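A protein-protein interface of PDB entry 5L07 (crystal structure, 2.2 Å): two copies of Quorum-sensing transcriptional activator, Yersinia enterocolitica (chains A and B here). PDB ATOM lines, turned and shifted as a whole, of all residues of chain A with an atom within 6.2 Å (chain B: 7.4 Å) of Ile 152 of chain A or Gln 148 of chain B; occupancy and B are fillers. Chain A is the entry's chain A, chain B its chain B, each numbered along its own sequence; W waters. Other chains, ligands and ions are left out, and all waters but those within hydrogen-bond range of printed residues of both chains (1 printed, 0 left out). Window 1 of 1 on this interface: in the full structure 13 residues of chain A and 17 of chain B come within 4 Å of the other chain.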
ATOM      1  N   LEU A 114      20.317   4.880  -8.718  1.00  0.00           N
ATOM      2  CA  LEU A 114      21.415   4.569  -7.817  1.00  0.00           C
ATOM      3  C   LEU A 114      22.735   4.672  -8.575  1.00  0.00           C
ATOM      4  O   LEU A 114      22.865   4.123  -9.673  1.00  0.00           O
ATOM      5  CB  LEU A 114      21.213   3.154  -7.255  1.00  0.00           C
ATOM      6  CG  LEU A 114      22.107   2.617  -6.169  1.00  0.00           C
ATOM      7  CD1 LEU A 114      22.021   3.555  -4.989  1.00  0.00           C
ATOM      8  CD2 LEU A 114      21.651   1.213  -5.788  1.00  0.00           C
ATOM      9  N   ILE A 147      10.562   0.973  -2.249  1.00  0.00           N
ATOM     10  CA  ILE A 147      11.019   0.596  -3.584  1.00  0.00           C
ATOM     11  C   ILE A 147      12.449   1.080  -3.820  1.00  0.00           C
ATOM     12  O   ILE A 147      13.256   0.380  -4.439  1.00  0.00           O
ATOM     13  CB  ILE A 147      10.043   1.145  -4.638  1.00  0.00           C
ATOM     14  CG1 ILE A 147       8.656   0.522  -4.428  1.00  0.00           C
ATOM     15  CG2 ILE A 147      10.566   0.886  -6.053  1.00  0.00           C
ATOM     16  CD1 ILE A 147       7.573   1.148  -5.306  1.00  0.00           C
ATOM     17  N   GLN A 148      12.789   2.278  -3.342  1.00  0.00           N
ATOM     18  CA  GLN A 148      14.184   2.710  -3.426  1.00  0.00           C
ATOM     19  C   GLN A 148      15.087   1.744  -2.679  1.00  0.00           C
ATOM     20  O   GLN A 148      16.169   1.387  -3.169  1.00  0.00           O
ATOM     21  CB  GLN A 148      14.373   4.125  -2.864  1.00  0.00           C
ATOM     22  CG  GLN A 148      15.845   4.576  -2.873  1.00  0.00           C
ATOM     23  CD  GLN A 148      16.323   4.947  -4.283  1.00  0.00           C
ATOM     24  OE1 GLN A 148      15.512   5.315  -5.129  1.00  0.00           O
ATOM     25  NE2 GLN A 148      17.636   4.888  -4.524  1.00  0.00           N
ATOM     26  N   MET A 149      14.659   1.305  -1.494  1.00  0.00           N
ATOM     27  CA  MET A 149      15.440   0.366  -0.721  1.00  0.00           C
ATOM     28  C   MET A 149      15.524  -0.979  -1.436  1.00  0.00           C
ATOM     29  O   MET A 149      16.543  -1.651  -1.366  1.00  0.00           O
ATOM     30  CB  MET A 149      14.849   0.182   0.689  1.00  0.00           C
ATOM     31  CG  MET A 149      15.735  -0.679   1.614  1.00  0.00           C
ATOM     32  SD  MET A 149      17.608  -0.082   1.776  1.00  0.00           S
ATOM     33  CE  MET A 149      17.334   1.625   2.690  1.00  0.00           C
ATOM     34  N   LEU A 150      14.465  -1.365  -2.142  1.00  0.00           N
ATOM     35  CA  LEU A 150      14.533  -2.603  -2.913  1.00  0.00           C
ATOM     36  C   LEU A 150      15.608  -2.511  -3.987  1.00  0.00           C
ATOM     37  O   LEU A 150      16.390  -3.450  -4.173  1.00  0.00           O
ATOM     38  CB  LEU A 150      13.173  -2.933  -3.535  1.00  0.00           C
ATOM     39  CG  LEU A 150      13.164  -4.122  -4.512  1.00  0.00           C
ATOM     40  CD1 LEU A 150      13.602  -5.445  -3.829  1.00  0.00           C
ATOM     41  CD2 LEU A 150      11.801  -4.285  -5.180  1.00  0.00           C
ATOM     42  N   LEU A 151      15.678  -1.377  -4.692  1.00  0.00           N
ATOM     43  CA  LEU A 151      16.743  -1.191  -5.679  1.00  0.00           C
ATOM     44  C   LEU A 151      18.123  -1.263  -5.029  1.00  0.00           C
ATOM     45  O   LEU A 151      19.023  -1.951  -5.535  1.00  0.00           O
ATOM     46  CB  LEU A 151      16.555   0.144  -6.413  1.00  0.00           C
ATOM     47  CG  LEU A 151      17.777   0.628  -7.209  1.00  0.00           C
ATOM     48  CD1 LEU A 151      18.134  -0.358  -8.341  1.00  0.00           C
ATOM     49  CD2 LEU A 151      17.527   2.025  -7.770  1.00  0.00           C
ATOM     50  N   ILE A 152      18.306  -0.569  -3.894  1.00  0.00           N
ATOM     51  CA  ILE A 152      19.585  -0.575  -3.177  1.00  0.00           C
ATOM     52  C   ILE A 152      20.014  -2.000  -2.803  1.00  0.00           C
ATOM     53  O   ILE A 152      21.188  -2.373  -2.941  1.00  0.00           O
ATOM     54  CB  ILE A 152      19.482   0.323  -1.930  1.00  0.00           C
ATOM     55  CG1 ILE A 152      19.531   1.807  -2.326  1.00  0.00           C
ATOM     56  CG2 ILE A 152      20.557  -0.011  -0.945  1.00  0.00           C
ATOM     57  CD1 ILE A 152      19.070   2.767  -1.215  1.00  0.00           C
ATOM     58  N   LEU A 153      19.078  -2.805  -2.289  1.00  0.00           N
ATOM     59  CA  LEU A 153      19.423  -4.136  -1.791  1.00  0.00           C
ATOM     60  C   LEU A 153      19.629  -5.119  -2.938  1.00  0.00           C
ATOM     61  O   LEU A 153      20.492  -5.999  -2.858  1.00  0.00           O
ATOM     62  CB  LEU A 153      18.332  -4.654  -0.841  1.00  0.00           C
ATOM     63  CG  LEU A 153      18.176  -3.957   0.520  1.00  0.00           C
ATOM     64  CD1 LEU A 153      17.012  -4.568   1.331  1.00  0.00           C
ATOM     65  CD2 LEU A 153      19.491  -4.025   1.316  1.00  0.00           C
ATOM     66  N   THR A 154      18.830  -4.996  -4.005  1.00  0.00           N
ATOM     67  CA  THR A 154      19.093  -5.745  -5.229  1.00  0.00           C
ATOM     68  C   THR A 154      20.496  -5.470  -5.747  1.00  0.00           C
ATOM     69  O   THR A 154      21.256  -6.394  -6.036  1.00  0.00           O
ATOM     70  CB  THR A 154      18.067  -5.393  -6.306  1.00  0.00           C
ATOM     71  OG1 THR A 154      16.752  -5.797  -5.886  1.00  0.00           O
ATOM     72  CG2 THR A 154      18.421  -6.108  -7.608  1.00  0.00           C
ATOM     73  N   HIS A 155      20.866  -4.195  -5.871  1.00  0.00           N
ATOM     74  CA  HIS A 155      22.189  -3.881  -6.394  1.00  0.00           C
ATOM     75  C   HIS A 155      23.293  -4.366  -5.455  1.00  0.00           C
ATOM     76  O   HIS A 155      24.304  -4.925  -5.908  1.00  0.00           O
ATOM     77  CB  HIS A 155      22.302  -2.378  -6.638  1.00  0.00           C
ATOM     78  CG  HIS A 155      23.501  -1.996  -7.439  1.00  0.00           C
ATOM     79  ND1 HIS A 155      23.544  -2.118  -8.812  1.00  0.00           N
ATOM     80  CD2 HIS A 155      24.707  -1.512  -7.062  1.00  0.00           C
ATOM     81  CE1 HIS A 155      24.726  -1.720  -9.246  1.00  0.00           C
ATOM     82  NE2 HIS A 155      25.451  -1.348  -8.204  1.00  0.00           N
ATOM     83  N   GLU A 156      23.126  -4.173  -4.146  1.00  0.00           N
ATOM     84  CA  GLU A 156      24.103  -4.717  -3.206  1.00  0.00           C
ATOM     85  C   GLU A 156      24.230  -6.228  -3.359  1.00  0.00           C
ATOM     86  O   GLU A 156      25.339  -6.779  -3.284  1.00  0.00           O
ATOM     87  CB  GLU A 156      23.714  -4.374  -1.769  1.00  0.00           C
ATOM     88  CG  GLU A 156      24.735  -4.894  -0.754  1.00  0.00           C
ATOM     89  CD  GLU A 156      24.209  -4.965   0.674  1.00  0.00           C
ATOM     90  OE1 GLU A 156      22.975  -5.061   0.866  1.00  0.00           O
ATOM     91  OE2 GLU A 156      25.041  -4.937   1.609  1.00  0.00           O
ATOM     92  N   LYS A 157      23.099  -6.916  -3.566  1.00  0.00           N
ATOM     93  CA  LYS A 157      23.140  -8.372  -3.712  1.00  0.00           C
ATOM     94  C   LYS A 157      23.817  -8.776  -5.018  1.00  0.00           C
ATOM     95  O   LYS A 157      24.586  -9.746  -5.050  1.00  0.00           O
ATOM     96  CB  LYS A 157      21.723  -8.952  -3.631  1.00  0.00           C
ATOM     97  CG  LYS A 157      21.650 -10.494  -3.645  1.00  0.00           C
ATOM     98  CD  LYS A 157      20.234 -10.979  -3.310  1.00  0.00           C
ATOM     99  CE  LYS A 157      19.964 -12.413  -3.789  1.00  0.00           C
ATOM    100  NZ  LYS A 157      20.591 -13.433  -2.921  1.00  0.00           N
ATOM    101  N   TYR B  26      12.793  10.149  14.318  1.00  0.00           N
ATOM    102  CA  TYR B  26      13.267   8.813  14.649  1.00  0.00           C
ATOM    103  C   TYR B  26      13.824   8.694  16.059  1.00  0.00           C
ATOM    104  O   TYR B  26      14.207   7.590  16.458  1.00  0.00           O
ATOM    105  CB  TYR B  26      14.295   8.375  13.612  1.00  0.00           C
ATOM    106  CG  TYR B  26      13.763   8.635  12.223  1.00  0.00           C
ATOM    107  CD1 TYR B  26      12.735   7.856  11.708  1.00  0.00           C
ATOM    108  CD2 TYR B  26      14.237   9.688  11.454  1.00  0.00           C
ATOM    109  CE1 TYR B  26      12.218   8.090  10.457  1.00  0.00           C
ATOM    110  CE2 TYR B  26      13.722   9.936  10.186  1.00  0.00           C
ATOM    111  CZ  TYR B  26      12.710   9.130   9.702  1.00  0.00           C
ATOM    112  OH  TYR B  26      12.180   9.349   8.452  1.00  0.00           O
ATOM    113  N   LYS B  76      30.122   0.911  -0.548  1.00  0.00           N
ATOM    114  CA  LYS B  76      28.797   0.354  -0.323  1.00  0.00           C
ATOM    115  C   LYS B  76      27.732   1.231  -0.956  1.00  0.00           C
ATOM    116  O   LYS B  76      27.970   2.401  -1.285  1.00  0.00           O
ATOM    117  CB  LYS B  76      28.508   0.188   1.171  1.00  0.00           C
ATOM    118  CG  LYS B  76      29.185  -1.033   1.780  1.00  0.00           C
ATOM    119  CD  LYS B  76      28.889  -1.125   3.261  1.00  0.00           C
ATOM    120  CE  LYS B  76      28.172  -2.411   3.619  1.00  0.00           C
ATOM    121  NZ  LYS B  76      26.818  -2.483   2.983  1.00  0.00           N
ATOM    122  N   VAL B  77      26.548   0.638  -1.132  1.00  0.00           N
ATOM    123  CA  VAL B  77      25.347   1.398  -1.443  1.00  0.00           C
ATOM    124  C   VAL B  77      24.263   1.226  -0.390  1.00  0.00           C
ATOM    125  O   VAL B  77      23.385   2.098  -0.277  1.00  0.00           O
ATOM    126  CB  VAL B  77      24.796   1.030  -2.850  1.00  0.00           C
ATOM    127  CG1 VAL B  77      25.803   1.432  -3.941  1.00  0.00           C
ATOM    128  CG2 VAL B  77      24.523  -0.486  -2.990  1.00  0.00           C
ATOM    129  N   ALA B  78      24.301   0.109   0.444  1.00  0.00           N
ATOM    130  CA  ALA B  78      23.236  -0.148   1.398  1.00  0.00           C
ATOM    131  C   ALA B  78      23.655   0.299   2.792  1.00  0.00           C
ATOM    132  O   ALA B  78      24.846   0.348   3.098  1.00  0.00           O
ATOM    133  CB  ALA B  78      22.877  -1.644   1.406  1.00  0.00           C
ATOM    134  N   PRO B  79      22.718   0.670   3.660  1.00  0.00           N
ATOM    135  CA  PRO B  79      23.109   1.124   5.005  1.00  0.00           C
ATOM    136  C   PRO B  79      23.731  -0.012   5.804  1.00  0.00           C
ATOM    137  O   PRO B  79      23.450  -1.186   5.572  1.00  0.00           O
ATOM    138  CB  PRO B  79      21.791   1.583   5.635  1.00  0.00           C
ATOM    139  CG  PRO B  79      20.798   1.677   4.482  1.00  0.00           C
ATOM    140  CD  PRO B  79      21.259   0.724   3.437  1.00  0.00           C
ATOM    141  N   THR B 111      25.368   3.974   9.384  1.00  0.00           N
ATOM    142  CA  THR B 111      25.694   4.856   8.275  1.00  0.00           C
ATOM    143  C   THR B 111      24.851   4.510   7.053  1.00  0.00           C
ATOM    144  O   THR B 111      24.757   3.345   6.655  1.00  0.00           O
ATOM    145  CB  THR B 111      27.187   4.797   7.928  1.00  0.00           C
ATOM    146  OG1 THR B 111      27.932   5.494   8.939  1.00  0.00           O
ATOM    147  CG2 THR B 111      27.458   5.495   6.554  1.00  0.00           C
ATOM    148  N   PHE B 112      24.247   5.541   6.470  1.00  0.00           N
ATOM    149  CA  PHE B 112      23.512   5.498   5.214  1.00  0.00           C
ATOM    150  C   PHE B 112      24.371   6.185   4.153  1.00  0.00           C
ATOM    151  O   PHE B 112      24.992   7.218   4.428  1.00  0.00           O
ATOM    152  CB  PHE B 112      22.153   6.210   5.384  1.00  0.00           C
ATOM    153  CG  PHE B 112      21.232   5.527   6.379  1.00  0.00           C
ATOM    154  CD1 PHE B 112      20.155   4.763   5.941  1.00  0.00           C
ATOM    155  CD2 PHE B 112      21.470   5.617   7.757  1.00  0.00           C
ATOM    156  CE1 PHE B 112      19.319   4.108   6.850  1.00  0.00           C
ATOM    157  CE2 PHE B 112      20.650   4.952   8.670  1.00  0.00           C
ATOM    158  CZ  PHE B 112      19.560   4.200   8.215  1.00  0.00           C
ATOM    159  N   VAL B 113      24.461   5.603   2.954  1.00  0.00           N
ATOM    160  CA  VAL B 113      25.426   6.114   1.984  1.00  0.00           C
ATOM    161  C   VAL B 113      24.742   6.369   0.649  1.00  0.00           C
ATOM    162  O   VAL B 113      23.740   5.734   0.295  1.00  0.00           O
ATOM    163  CB  VAL B 113      26.658   5.172   1.825  1.00  0.00           C
ATOM    164  CG1 VAL B 113      26.251   3.765   1.415  1.00  0.00           C
ATOM    165  CG2 VAL B 113      27.680   5.765   0.855  1.00  0.00           C
ATOM    166  N   LEU B 114      25.268   7.357  -0.072  1.00  0.00           N
ATOM    167  CA  LEU B 114      24.784   7.720  -1.387  1.00  0.00           C
ATOM    168  C   LEU B 114      25.978   8.131  -2.243  1.00  0.00           C
ATOM    169  O   LEU B 114      26.784   8.960  -1.816  1.00  0.00           O
ATOM    170  CB  LEU B 114      23.773   8.870  -1.263  1.00  0.00           C
ATOM    171  CG  LEU B 114      23.124   9.555  -2.447  1.00  0.00           C
ATOM    172  CD1 LEU B 114      22.017  10.433  -1.932  1.00  0.00           C
ATOM    173  CD2 LEU B 114      24.125  10.434  -3.158  1.00  0.00           C
ATOM    174  N   HIS B 115      26.068   7.598  -3.458  1.00  0.00           N
ATOM    175  CA  HIS B 115      27.036   8.068  -4.440  1.00  0.00           C
ATOM    176  C   HIS B 115      26.298   8.769  -5.571  1.00  0.00           C
ATOM    177  O   HIS B 115      25.255   8.296  -6.016  1.00  0.00           O
ATOM    178  CB  HIS B 115      27.863   6.913  -5.000  1.00  0.00           C
ATOM    179  CG  HIS B 115      28.619   6.157  -3.961  1.00  0.00           C
ATOM    180  ND1 HIS B 115      29.971   6.324  -3.755  1.00  0.00           N
ATOM    181  CD2 HIS B 115      28.210   5.235  -3.056  1.00  0.00           C
ATOM    182  CE1 HIS B 115      30.362   5.540  -2.765  1.00  0.00           C
ATOM    183  NE2 HIS B 115      29.311   4.869  -2.321  1.00  0.00           N
ATOM    184  N   ALA B 122      28.036  10.906  -0.267  1.00  0.00           N
ATOM    185  CA  ALA B 122      27.354  11.544   0.859  1.00  0.00           C
ATOM    186  C   ALA B 122      26.993  10.462   1.865  1.00  0.00           C
ATOM    187  O   ALA B 122      26.516   9.395   1.478  1.00  0.00           O
ATOM    188  CB  ALA B 122      26.095  12.288   0.386  1.00  0.00           C
ATOM    189  N   LEU B 124      25.102   9.832   5.804  1.00  0.00           N
ATOM    190  CA  LEU B 124      24.378  10.290   6.985  1.00  0.00           C
ATOM    191  C   LEU B 124      24.693   9.270   8.075  1.00  0.00           C
ATOM    192  O   LEU B 124      24.322   8.095   7.965  1.00  0.00           O
ATOM    193  CB  LEU B 124      22.873  10.414   6.708  1.00  0.00           C
ATOM    194  CG  LEU B 124      21.926  10.692   7.885  1.00  0.00           C
ATOM    195  CD1 LEU B 124      22.259  12.034   8.510  1.00  0.00           C
ATOM    196  CD2 LEU B 124      20.438  10.661   7.443  1.00  0.00           C
ATOM    197  N   ASN B 143      12.784   2.079  10.483  1.00  0.00           N
ATOM    198  CA  ASN B 143      12.691   3.281   9.653  1.00  0.00           C
ATOM    199  C   ASN B 143      13.819   3.403   8.635  1.00  0.00           C
ATOM    200  O   ASN B 143      14.006   4.474   8.045  1.00  0.00           O
ATOM    201  CB  ASN B 143      12.670   4.509  10.557  1.00  0.00           C
ATOM    202  CG  ASN B 143      11.436   4.541  11.434  1.00  0.00           C
ATOM    203  OD1 ASN B 143      10.327   4.518  10.922  1.00  0.00           O
ATOM    204  ND2 ASN B 143      11.622   4.537  12.747  1.00  0.00           N
ATOM    205  N   LYS B 144      14.561   2.323   8.413  1.00  0.00           N
ATOM    206  CA  LYS B 144      15.730   2.328   7.537  1.00  0.00           C
ATOM    207  C   LYS B 144      15.435   2.939   6.164  1.00  0.00           C
ATOM    208  O   LYS B 144      16.256   3.696   5.611  1.00  0.00           O
ATOM    209  CB  LYS B 144      16.206   0.878   7.396  1.00  0.00           C
ATOM    210  CG  LYS B 144      17.526   0.694   6.759  1.00  0.00           C
ATOM    211  CD  LYS B 144      17.825  -0.790   6.566  1.00  0.00           C
ATOM    212  CE  LYS B 144      16.895  -1.407   5.534  1.00  0.00           C
ATOM    213  NZ  LYS B 144      17.091  -2.880   5.402  1.00  0.00           N
ATOM    214  N   GLU B 145      14.298   2.580   5.572  1.00  0.00           N
ATOM    215  CA  GLU B 145      13.971   3.062   4.232  1.00  0.00           C
ATOM    216  C   GLU B 145      13.688   4.559   4.249  1.00  0.00           C
ATOM    217  O   GLU B 145      14.020   5.274   3.286  1.00  0.00           O
ATOM    218  CB  GLU B 145      12.759   2.318   3.669  1.00  0.00           C
ATOM    219  CG  GLU B 145      12.890   0.809   3.684  1.00  0.00           C
ATOM    220  CD  GLU B 145      12.567   0.191   5.041  1.00  0.00           C
ATOM    221  OE1 GLU B 145      12.090   0.918   5.946  1.00  0.00           O
ATOM    222  OE2 GLU B 145      12.800  -1.029   5.200  1.00  0.00           O
ATOM    223  N   LYS B 146      13.054   5.042   5.323  1.00  0.00           N
ATOM    224  CA  LYS B 146      12.722   6.463   5.406  1.00  0.00           C
ATOM    225  C   LYS B 146      13.970   7.303   5.625  1.00  0.00           C
ATOM    226  O   LYS B 146      14.079   8.405   5.076  1.00  0.00           O
ATOM    227  CB  LYS B 146      11.703   6.708   6.525  1.00  0.00           C
ATOM    228  CG  LYS B 146      10.381   5.995   6.292  1.00  0.00           C
ATOM    229  CD  LYS B 146       9.385   6.235   7.418  1.00  0.00           C
ATOM    230  CE  LYS B 146       8.064   5.502   7.139  1.00  0.00           C
ATOM    231  NZ  LYS B 146       7.120   5.616   8.287  1.00  0.00           N
ATOM    232  N   ILE B 147      14.931   6.793   6.410  1.00  0.00           N
ATOM    233  CA  ILE B 147      16.141   7.563   6.686  1.00  0.00           C
ATOM    234  C   ILE B 147      17.019   7.636   5.440  1.00  0.00           C
ATOM    235  O   ILE B 147      17.665   8.656   5.175  1.00  0.00           O
ATOM    236  CB  ILE B 147      16.903   6.959   7.881  1.00  0.00           C
ATOM    237  CG1 ILE B 147      16.007   6.902   9.125  1.00  0.00           C
ATOM    238  CG2 ILE B 147      18.178   7.778   8.182  1.00  0.00           C
ATOM    239  CD1 ILE B 147      16.579   6.033  10.263  1.00  0.00           C
ATOM    240  N   GLN B 148      17.078   6.549   4.673  1.00  0.00           N
ATOM    241  CA  GLN B 148      17.766   6.577   3.388  1.00  0.00           C
ATOM    242  C   GLN B 148      17.148   7.620   2.455  1.00  0.00           C
ATOM    243  O   GLN B 148      17.866   8.313   1.722  1.00  0.00           O
ATOM    244  CB  GLN B 148      17.714   5.187   2.733  1.00  0.00           C
ATOM    245  CG  GLN B 148      18.376   5.133   1.364  1.00  0.00           C
ATOM    246  CD  GLN B 148      19.917   5.236   1.459  1.00  0.00           C
ATOM    247  OE1 GLN B 148      20.496   4.914   2.500  1.00  0.00           O
ATOM    248  NE2 GLN B 148      20.575   5.662   0.365  1.00  0.00           N
ATOM    249  N   MET B 149      15.815   7.730   2.446  1.00  0.00           N
ATOM    250  CA  MET B 149      15.160   8.731   1.598  1.00  0.00           C
ATOM    251  C   MET B 149      15.482  10.141   2.099  1.00  0.00           C
ATOM    252  O   MET B 149      15.655  11.078   1.290  1.00  0.00           O
ATOM    253  CB  MET B 149      13.636   8.522   1.539  1.00  0.00           C
ATOM    254  CG  MET B 149      12.930   9.426   0.493  1.00  0.00           C
ATOM    255  SD  MET B 149      13.663   9.276  -1.361  1.00  0.00           S
ATOM    256  CE  MET B 149      13.047   7.468  -1.735  1.00  0.00           C
ATOM    257  N   LEU B 150      15.590  10.306   3.424  1.00  0.00           N
ATOM    258  CA  LEU B 150      16.015  11.604   3.944  1.00  0.00           C
ATOM    259  C   LEU B 150      17.404  11.974   3.429  1.00  0.00           C
ATOM    260  O   LEU B 150      17.646  13.131   3.052  1.00  0.00           O
ATOM    261  CB  LEU B 150      16.004  11.609   5.473  1.00  0.00           C
ATOM    262  CG  LEU B 150      16.459  12.921   6.124  1.00  0.00           C
ATOM    263  CD1 LEU B 150      15.484  14.047   5.747  1.00  0.00           C
ATOM    264  CD2 LEU B 150      16.509  12.760   7.648  1.00  0.00           C
ATOM    265  N   LEU B 151      18.340  11.013   3.435  1.00  0.00           N
ATOM    266  CA  LEU B 151      19.658  11.277   2.872  1.00  0.00           C
ATOM    267  C   LEU B 151      19.553  11.691   1.409  1.00  0.00           C
ATOM    268  O   LEU B 151      20.211  12.650   0.974  1.00  0.00           O
ATOM    269  CB  LEU B 151      20.558  10.046   3.009  1.00  0.00           C
ATOM    270  CG  LEU B 151      21.891  10.014   2.231  1.00  0.00           C
ATOM    271  CD1 LEU B 151      22.793  11.260   2.476  1.00  0.00           C
ATOM    272  CD2 LEU B 151      22.683   8.736   2.550  1.00  0.00           C
ATOM    273  N   ILE B 152      18.717  10.988   0.638  1.00  0.00           N
ATOM    274  CA  ILE B 152      18.600  11.254  -0.796  1.00  0.00           C
ATOM    275  C   ILE B 152      18.013  12.644  -1.043  1.00  0.00           C
ATOM    276  O   ILE B 152      18.488  13.396  -1.915  1.00  0.00           O
ATOM    277  CB  ILE B 152      17.748  10.147  -1.448  1.00  0.00           C
ATOM    278  CG1 ILE B 152      18.511   8.812  -1.484  1.00  0.00           C
ATOM    279  CG2 ILE B 152      17.294  10.516  -2.866  1.00  0.00           C
ATOM    280  CD1 ILE B 152      17.583   7.606  -1.857  1.00  0.00           C
ATOM    281  N   LEU B 153      16.982  13.016  -0.286  1.00  0.00           N
ATOM    282  CA  LEU B 153      16.337  14.303  -0.536  1.00  0.00           C
ATOM    283  C   LEU B 153      17.181  15.459  -0.014  1.00  0.00           C
ATOM    284  O   LEU B 153      17.146  16.543  -0.598  1.00  0.00           O
ATOM    285  CB  LEU B 153      14.937  14.329   0.078  1.00  0.00           C
ATOM    286  CG  LEU B 153      13.931  13.369  -0.580  1.00  0.00           C
ATOM    287  CD1 LEU B 153      12.604  13.335   0.164  1.00  0.00           C
ATOM    288  CD2 LEU B 153      13.690  13.751  -2.033  1.00  0.00           C
ATOM    289  N   THR B 154      17.947  15.244   1.062  1.00  0.00           N
ATOM    290  CA  THR B 154      18.906  16.246   1.529  1.00  0.00           C
ATOM    291  C   THR B 154      19.974  16.508   0.482  1.00  0.00           C
ATOM    292  O   THR B 154      20.287  17.661   0.171  1.00  0.00           O
ATOM    293  CB  THR B 154      19.584  15.775   2.820  1.00  0.00           C
ATOM    294  OG1 THR B 154      18.603  15.613   3.845  1.00  0.00           O
ATOM    295  CG2 THR B 154      20.641  16.810   3.272  1.00  0.00           C
HETATM  296  O   HOH W   1      20.191   5.546  -2.751  1.00  0.00           O
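The side-chain carboxylate (OE2) of Glu 156 of chain A is in salt-bridge range of the side-chain amino group (NZ) of Lys 76 of chain B.
O of Ala 78 of chain B is in hydrogen-bond range of NZ of Lys 76 of chain B (3.5 Å).
The backbone carbonyl oxygen of Lys 76 of chain B is in hydrogen-bond range of a ring nitrogen (NE2) of His 115 of chain B (3.0 Å).
The backbone carbonyl oxygen (O) of Val 113 of chain B sits at hydrogen-bond distance from the side-chain amide nitrogen (NE2) of Gln 148 of chain B.
Among the printed residues, merely in contact across the chains: Glu 156 of chain A with Ala 78 of chain B, Ile 152 of chain A with Ala 78 of chain B, Ile 152 of chain A with Gln 148 of chain B, Met 149 of chain A with Gln 148 of chain B, Ile 152 of chain A with Val 77 of chain B, Met 149 of chain A with Glu 145 of chain B, Gln 148 of chain A with Ile 152 of chain B, Met 149 of chain A with Lys 144 of chain B, Gln 148 of chain A with Met 149 of chain B and Met 149 of chain A with Pro 79 of chain B.
Ile 152 of chain A touches three residues of chain B.
Gln 148 of chain B touches two residues of chain A.
Of the printed residues of chain A, Glu 145 of chain B touches Met 149 (3.6 Å).
Of the printed residues of chain B, Glu 156 of chain A touches Lys 76 and Ala 78.
Printed residues of chain A within 4 Å of Val 77 of chain B: Ile 152 (3.6 Å).
Of the printed residues of chain B, Gln 148 of chain A touches Met 149 and Ile 152.
Tyr 26 of chain B touches none of the printed residues of chain A.
Leu 153 of chain B touches none of the printed residues of chain A.
The nearest residue of chain B that does not touch Ile 152 of chain A is Pro 79 of chain B (4.5 Å).
The nearest residue of chain A that does not touch Gln 148 of chain B is Gln 148 of chain A (5.0 Å).
The nearest printed residue of chain B that does not touch Met 149 of chain A is Phe 112 of chain B (5.2 Å).
Hydrophobic or aromatic side chains of chain B within 4 Å of the printed part of chain A: Val 77, Ala 78, Pro 79, Met 149 and Ile 152.
Printed residues of chain A that touch a printed residue of chain B: Gln 148, Met 149, Ile 152 and Glu 156.
Along chain A the printed residues that touch a printed residue of chain B span positions 148 to 156.
Gln 148 of chain A touches Met 149 of chain B, and with the chains exchanged Met 149 of chain A touches Gln 148 of chain B.
Gln 148 of chain A touches Ile 152 of chain B, and with the chains exchanged Ile 152 of chain A touches Gln 148 of chain B.
9 positions are printed for both chains.
Of the 11 pairs that touch across the chains among the printed residues, 4 have their exchanged pair printed and touching as well.
Water W1 lies within hydrogen-bond range of the side-chain amide nitrogen of Gln 148 of chain B (3.1 Å) and the side-chain amide nitrogen of Gln 148 of chain A (3.2 Å).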
